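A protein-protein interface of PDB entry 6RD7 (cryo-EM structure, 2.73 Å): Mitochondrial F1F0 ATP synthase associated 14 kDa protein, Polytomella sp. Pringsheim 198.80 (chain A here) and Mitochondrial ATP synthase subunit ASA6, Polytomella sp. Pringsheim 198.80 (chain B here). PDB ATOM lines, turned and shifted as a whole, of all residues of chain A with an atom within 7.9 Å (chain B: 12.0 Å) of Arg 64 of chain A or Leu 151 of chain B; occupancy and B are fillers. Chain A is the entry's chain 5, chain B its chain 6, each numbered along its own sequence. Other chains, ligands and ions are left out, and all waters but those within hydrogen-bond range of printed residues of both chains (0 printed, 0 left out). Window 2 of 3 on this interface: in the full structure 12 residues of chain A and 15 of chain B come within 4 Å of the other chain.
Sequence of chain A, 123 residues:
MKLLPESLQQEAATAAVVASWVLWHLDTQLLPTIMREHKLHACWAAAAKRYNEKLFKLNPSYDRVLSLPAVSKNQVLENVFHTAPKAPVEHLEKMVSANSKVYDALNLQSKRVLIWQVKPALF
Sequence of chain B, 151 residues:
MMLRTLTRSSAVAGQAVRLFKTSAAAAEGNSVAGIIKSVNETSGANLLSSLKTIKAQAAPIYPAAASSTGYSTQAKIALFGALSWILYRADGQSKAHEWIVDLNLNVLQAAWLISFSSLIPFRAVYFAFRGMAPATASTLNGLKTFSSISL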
ATOM      1  N   ASN A  59      -9.908   1.443   7.644  1.00  0.00           N
ATOM      2  CA  ASN A  59     -10.724   1.813   6.495  1.00  0.00           C
ATOM      3  C   ASN A  59      -9.910   1.753   5.211  1.00  0.00           C
ATOM      4  O   ASN A  59      -8.934   2.501   5.081  1.00  0.00           O
ATOM      5  CB  ASN A  59     -11.279   3.215   6.702  1.00  0.00           C
ATOM      6  CG  ASN A  59     -12.546   3.462   5.934  1.00  0.00           C
ATOM      7  OD1 ASN A  59     -12.956   2.651   5.113  1.00  0.00           O
ATOM      8  ND2 ASN A  59     -13.176   4.596   6.192  1.00  0.00           N
ATOM      9  N   PRO A  60     -10.255   0.898   4.249  1.00  0.00           N
ATOM     10  CA  PRO A  60      -9.523   0.860   2.970  1.00  0.00           C
ATOM     11  C   PRO A  60     -10.050   1.817   1.908  1.00  0.00           C
ATOM     12  O   PRO A  60      -9.687   1.655   0.742  1.00  0.00           O
ATOM     13  CB  PRO A  60      -9.740  -0.590   2.532  1.00  0.00           C
ATOM     14  CG  PRO A  60     -11.098  -0.917   3.038  1.00  0.00           C
ATOM     15  CD  PRO A  60     -11.339  -0.099   4.279  1.00  0.00           C
ATOM     16  N   SER A  61     -10.868   2.799   2.284  1.00  0.00           N
ATOM     17  CA  SER A  61     -11.598   3.580   1.294  1.00  0.00           C
ATOM     18  C   SER A  61     -10.741   4.689   0.701  1.00  0.00           C
ATOM     19  O   SER A  61     -11.028   5.183  -0.393  1.00  0.00           O
ATOM     20  CB  SER A  61     -12.850   4.169   1.935  1.00  0.00           C
ATOM     21  OG  SER A  61     -13.825   3.168   2.146  1.00  0.00           O
ATOM     22  N   TYR A  62      -9.685   5.093   1.401  1.00  0.00           N
ATOM     23  CA  TYR A  62      -8.979   6.309   1.013  1.00  0.00           C
ATOM     24  C   TYR A  62      -8.005   6.058  -0.129  1.00  0.00           C
ATOM     25  O   TYR A  62      -7.847   6.905  -1.013  1.00  0.00           O
ATOM     26  CB  TYR A  62      -8.258   6.888   2.221  1.00  0.00           C
ATOM     27  CG  TYR A  62      -9.145   6.976   3.428  1.00  0.00           C
ATOM     28  CD1 TYR A  62     -10.212   7.861   3.460  1.00  0.00           C
ATOM     29  CD2 TYR A  62      -8.927   6.166   4.526  1.00  0.00           C
ATOM     30  CE1 TYR A  62     -11.030   7.941   4.559  1.00  0.00           C
ATOM     31  CE2 TYR A  62      -9.736   6.239   5.624  1.00  0.00           C
ATOM     32  CZ  TYR A  62     -10.785   7.126   5.637  1.00  0.00           C
ATOM     33  OH  TYR A  62     -11.595   7.194   6.738  1.00  0.00           O
ATOM     34  N   ASP A  63      -7.343   4.905  -0.130  1.00  0.00           N
ATOM     35  CA  ASP A  63      -6.392   4.557  -1.181  1.00  0.00           C
ATOM     36  C   ASP A  63      -6.977   3.545  -2.157  1.00  0.00           C
ATOM     37  O   ASP A  63      -6.290   2.619  -2.594  1.00  0.00           O
ATOM     38  CB  ASP A  63      -5.089   4.042  -0.578  1.00  0.00           C
ATOM     39  CG  ASP A  63      -5.309   3.068   0.558  1.00  0.00           C
ATOM     40  OD1 ASP A  63      -6.477   2.805   0.909  1.00  0.00           O
ATOM     41  OD2 ASP A  63      -4.306   2.565   1.104  1.00  0.00           O
ATOM     42  N   ARG A  64      -8.259   3.699  -2.497  1.00  0.00           N
ATOM     43  CA  ARG A  64      -8.880   2.841  -3.501  1.00  0.00           C
ATOM     44  C   ARG A  64      -8.329   3.129  -4.889  1.00  0.00           C
ATOM     45  O   ARG A  64      -8.324   2.249  -5.757  1.00  0.00           O
ATOM     46  CB  ARG A  64     -10.394   3.037  -3.497  1.00  0.00           C
ATOM     47  CG  ARG A  64     -11.101   2.415  -2.325  1.00  0.00           C
ATOM     48  CD  ARG A  64     -11.156   0.913  -2.440  1.00  0.00           C
ATOM     49  NE  ARG A  64     -12.199   0.368  -1.581  1.00  0.00           N
ATOM     50  CZ  ARG A  64     -12.082  -0.755  -0.887  1.00  0.00           C
ATOM     51  NH1 ARG A  64     -10.964  -1.461  -0.945  1.00  0.00           N
ATOM     52  NH2 ARG A  64     -13.085  -1.171  -0.130  1.00  0.00           N
ATOM     53  N   VAL A  65      -7.860   4.359  -5.111  1.00  0.00           N
ATOM     54  CA  VAL A  65      -7.348   4.782  -6.412  1.00  0.00           C
ATOM     55  C   VAL A  65      -6.038   4.076  -6.746  1.00  0.00           C
ATOM     56  O   VAL A  65      -5.676   3.936  -7.919  1.00  0.00           O
ATOM     57  CB  VAL A  65      -7.211   6.324  -6.422  1.00  0.00           C
ATOM     58  CG1 VAL A  65      -6.077   6.797  -5.519  1.00  0.00           C
ATOM     59  CG2 VAL A  65      -7.061   6.867  -7.828  1.00  0.00           C
ATOM     60  N   LEU A  66      -5.334   3.575  -5.733  1.00  0.00           N
ATOM     61  CA  LEU A  66      -4.047   2.940  -5.970  1.00  0.00           C
ATOM     62  C   LEU A  66      -4.209   1.472  -6.330  1.00  0.00           C
ATOM     63  O   LEU A  66      -3.245   0.819  -6.746  1.00  0.00           O
ATOM     64  CB  LEU A  66      -3.168   3.102  -4.739  1.00  0.00           C
ATOM     65  CG  LEU A  66      -2.868   4.527  -4.290  1.00  0.00           C
ATOM     66  CD1 LEU A  66      -1.954   4.508  -3.088  1.00  0.00           C
ATOM     67  CD2 LEU A  66      -2.246   5.313  -5.420  1.00  0.00           C
ATOM     68  N   SER A  67      -5.410   0.929  -6.167  1.00  0.00           N
ATOM     69  CA  SER A  67      -5.703  -0.429  -6.602  1.00  0.00           C
ATOM     70  C   SER A  67      -6.191  -0.481  -8.039  1.00  0.00           C
ATOM     71  O   SER A  67      -6.364  -1.575  -8.583  1.00  0.00           O
ATOM     72  CB  SER A  67      -6.741  -1.065  -5.678  1.00  0.00           C
ATOM     73  OG  SER A  67      -6.264  -1.123  -4.347  1.00  0.00           O
ATOM     74  N   LEU A  68      -6.409   0.670  -8.655  1.00  0.00           N
ATOM     75  CA  LEU A  68      -6.858   0.824 -10.029  1.00  0.00           C
ATOM     76  C   LEU A  68      -5.661   0.637 -10.956  1.00  0.00           C
ATOM     77  O   LEU A  68      -4.519   0.682 -10.482  1.00  0.00           O
ATOM     78  CB  LEU A  68      -7.503   2.204 -10.196  1.00  0.00           C
ATOM     79  CG  LEU A  68      -9.032   2.275 -10.172  1.00  0.00           C
ATOM     80  CD1 LEU A  68      -9.594   1.786  -8.853  1.00  0.00           C
ATOM     81  CD2 LEU A  68      -9.486   3.696 -10.440  1.00  0.00           C
ATOM     82  N   PRO A  69      -5.860   0.388 -12.255  1.00  0.00           N
ATOM     83  CA  PRO A  69      -4.718   0.365 -13.185  1.00  0.00           C
ATOM     84  C   PRO A  69      -4.111   1.754 -13.315  1.00  0.00           C
ATOM     85  O   PRO A  69      -4.819   2.737 -13.544  1.00  0.00           O
ATOM     86  CB  PRO A  69      -5.344  -0.106 -14.502  1.00  0.00           C
ATOM     87  CG  PRO A  69      -6.792   0.183 -14.355  1.00  0.00           C
ATOM     88  CD  PRO A  69      -7.084  -0.083 -12.923  1.00  0.00           C
ATOM     89  N   ILE B  36     -29.401  -1.737   1.963  1.00  0.00           N
ATOM     90  CA  ILE B  36     -28.541  -2.382   0.974  1.00  0.00           C
ATOM     91  C   ILE B  36     -29.346  -3.335   0.100  1.00  0.00           C
ATOM     92  O   ILE B  36     -29.238  -3.305  -1.133  1.00  0.00           O
ATOM     93  CB  ILE B  36     -27.377  -3.097   1.685  1.00  0.00           C
ATOM     94  CG1 ILE B  36     -26.394  -2.074   2.250  1.00  0.00           C
ATOM     95  CG2 ILE B  36     -26.663  -4.053   0.753  1.00  0.00           C
ATOM     96  CD1 ILE B  36     -25.397  -2.660   3.211  1.00  0.00           C
ATOM     97  N   THR B 145     -17.091  11.467  10.925  1.00  0.00           N
ATOM     98  CA  THR B 145     -17.553  10.960   9.639  1.00  0.00           C
ATOM     99  C   THR B 145     -16.389  10.480   8.780  1.00  0.00           C
ATOM    100  O   THR B 145     -16.476   9.424   8.146  1.00  0.00           O
ATOM    101  CB  THR B 145     -18.357  12.043   8.921  1.00  0.00           C
ATOM    102  OG1 THR B 145     -19.510  12.379   9.698  1.00  0.00           O
ATOM    103  CG2 THR B 145     -18.815  11.576   7.552  1.00  0.00           C
ATOM    104  N   PHE B 146     -15.269  11.211   8.807  1.00  0.00           N
ATOM    105  CA  PHE B 146     -14.159  10.951   7.891  1.00  0.00           C
ATOM    106  C   PHE B 146     -13.469   9.621   8.174  1.00  0.00           C
ATOM    107  O   PHE B 146     -12.821   9.056   7.288  1.00  0.00           O
ATOM    108  CB  PHE B 146     -13.140  12.084   7.975  1.00  0.00           C
ATOM    109  CG  PHE B 146     -13.262  13.101   6.883  1.00  0.00           C
ATOM    110  CD1 PHE B 146     -12.549  12.964   5.708  1.00  0.00           C
ATOM    111  CD2 PHE B 146     -14.082  14.199   7.033  1.00  0.00           C
ATOM    112  CE1 PHE B 146     -12.653  13.911   4.709  1.00  0.00           C
ATOM    113  CE2 PHE B 146     -14.181  15.149   6.040  1.00  0.00           C
ATOM    114  CZ  PHE B 146     -13.475  15.000   4.875  1.00  0.00           C
ATOM    115  N   SER B 147     -13.584   9.106   9.399  1.00  0.00           N
ATOM    116  CA  SER B 147     -12.992   7.807   9.697  1.00  0.00           C
ATOM    117  C   SER B 147     -13.888   6.671   9.226  1.00  0.00           C
ATOM    118  O   SER B 147     -13.404   5.581   8.906  1.00  0.00           O
ATOM    119  CB  SER B 147     -12.715   7.680  11.190  1.00  0.00           C
ATOM    120  OG  SER B 147     -13.918   7.684  11.926  1.00  0.00           O
ATOM    121  N   SER B 148     -15.196   6.905   9.176  1.00  0.00           N
ATOM    122  CA  SER B 148     -16.162   5.873   8.838  1.00  0.00           C
ATOM    123  C   SER B 148     -16.733   6.027   7.437  1.00  0.00           C
ATOM    124  O   SER B 148     -17.815   5.501   7.164  1.00  0.00           O
ATOM    125  CB  SER B 148     -17.300   5.869   9.857  1.00  0.00           C
ATOM    126  OG  SER B 148     -18.109   7.019   9.708  1.00  0.00           O
ATOM    127  N   ILE B 149     -16.043   6.744   6.549  1.00  0.00           N
ATOM    128  CA  ILE B 149     -16.511   6.870   5.176  1.00  0.00           C
ATOM    129  C   ILE B 149     -16.274   5.562   4.440  1.00  0.00           C
ATOM    130  O   ILE B 149     -15.166   5.012   4.443  1.00  0.00           O
ATOM    131  CB  ILE B 149     -15.821   8.056   4.479  1.00  0.00           C
ATOM    132  CG1 ILE B 149     -16.481   9.362   4.900  1.00  0.00           C
ATOM    133  CG2 ILE B 149     -15.888   7.936   2.972  1.00  0.00           C
ATOM    134  CD1 ILE B 149     -15.746  10.585   4.462  1.00  0.00           C
ATOM    135  N   SER B 150     -17.330   5.046   3.816  1.00  0.00           N
ATOM    136  CA  SER B 150     -17.279   3.800   3.069  1.00  0.00           C
ATOM    137  C   SER B 150     -17.251   4.102   1.580  1.00  0.00           C
ATOM    138  O   SER B 150     -18.195   4.695   1.054  1.00  0.00           O
ATOM    139  CB  SER B 150     -18.483   2.915   3.397  1.00  0.00           C
ATOM    140  OG  SER B 150     -18.461   1.731   2.622  1.00  0.00           O
ATOM    141  N   LEU B 151     -16.156   3.721   0.922  1.00  0.00           N
ATOM    142  CA  LEU B 151     -16.059   3.657  -0.539  1.00  0.00           C
ATOM    143  C   LEU B 151     -14.836   2.819  -0.901  1.00  0.00           C
ATOM    144  O   LEU B 151     -14.475   2.695  -2.068  1.00  0.00           O
ATOM    145  CB  LEU B 151     -15.980   5.054  -1.183  1.00  0.00           C
ATOM    146  CG  LEU B 151     -14.829   6.042  -0.977  1.00  0.00           C
ATOM    147  CD1 LEU B 151     -13.776   5.930  -2.069  1.00  0.00           C
ATOM    148  CD2 LEU B 151     -15.358   7.455  -0.916  1.00  0.00           C
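OG of Ser 61 of chain A lies within hydrogen-bond range of N of Leu 151 of chain B.
The backbone carbonyl oxygen (O) of Phe 146 of chain B sits close to the side-chain hydroxyl (OH) of Tyr 62 of chain A, 2.3 Å away.
The side-chain amide nitrogen (ND2) of Asn 59 of chain A is in hydrogen-bond range of the backbone carbonyl oxygen (O) of Ser 147 of chain B.
The backbone carbonyl oxygen of Ile 149 of chain B is in hydrogen-bond range of the side-chain hydroxyl of Ser 61 of chain A (3.2 Å).
The side-chain hydroxyl (OH) of Tyr 62 of chain A sits at hydrogen-bond distance from the backbone carbonyl oxygen (O) of Ser 147 of chain B.
O of Ile 149 of chain B lies within hydrogen-bond range of ND2 of Asn 59 of chain A (2.7 Å).
The backbone carbonyl oxygen of Leu 151 of chain B lies within hydrogen-bond range of the guanidinium group of Arg 64 of chain A, at 3.3 Å.
The side-chain amide nitrogen of Asn 59 of chain A lies within hydrogen-bond range of the side-chain hydroxyl of Tyr 62 of chain A (3.1 Å).
OG of Ser 61 of chain A is in hydrogen-bond range of OD1 of Asn 59 of chain A, 3.1 Å away.
Among the printed residues, merely in contact across the chains: Ser 61 of chain A with Ser 150 of chain B (3.6 Å).
Printed residues of chain B within 4 Å of Asn 59 of chain A: Ser 147 and Ile 149.
Ser 61 of chain A touches just these residues of chain B: Ile 149, Ser 150 and Leu 151.
Printed residues of chain B within 4 Å of Tyr 62 of chain A: Phe 146 (2.3 Å) and Ser 147 (3.3 Å).
No residue of chain B comes within 4 Å of Asp 63 of chain A.
Of chain B, only Leu 151 (3.3 Å) comes within 4 Å of Arg 64 of chain A.
No residue of chain B comes within 4 Å of Val 65 of chain A.
No residue of chain B comes within 4 Å of Leu 66 of chain A.
No residue of chain B comes within 4 Å of Ser 67 of chain A.
Ile 36 of chain B touches none of the printed residues of chain A.
Of the printed residues of chain A, Ser 147 of chain B touches Asn 59 and Tyr 62.
Of the printed residues of chain A, Ile 149 of chain B touches Asn 59 (2.7 Å) and Ser 61 (3.2 Å).
Ser 150 of chain B touches just one residue of chain A: Ser 61 (3.6 Å).
Leu 151 of chain B touches just these residues of chain A: Ser 61 (2.7 Å) and Arg 64 (3.3 Å).
Hydrophobic or aromatic side chains of chain B within 4 Å of the printed part of chain A: Leu 151.
Hydrophobic or aromatic side chains of chain A that line the printed part of chain B: Tyr 62.
Along chain A the printed residues that touch a printed residue of chain B span positions 59 to 64.
Among the printed residues, 8 pairs touch across the chains.
Among the printed residues, no Asp or Glu carboxylate lies within 4 Å of a Lys or Arg side-chain nitrogen of the other chain.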
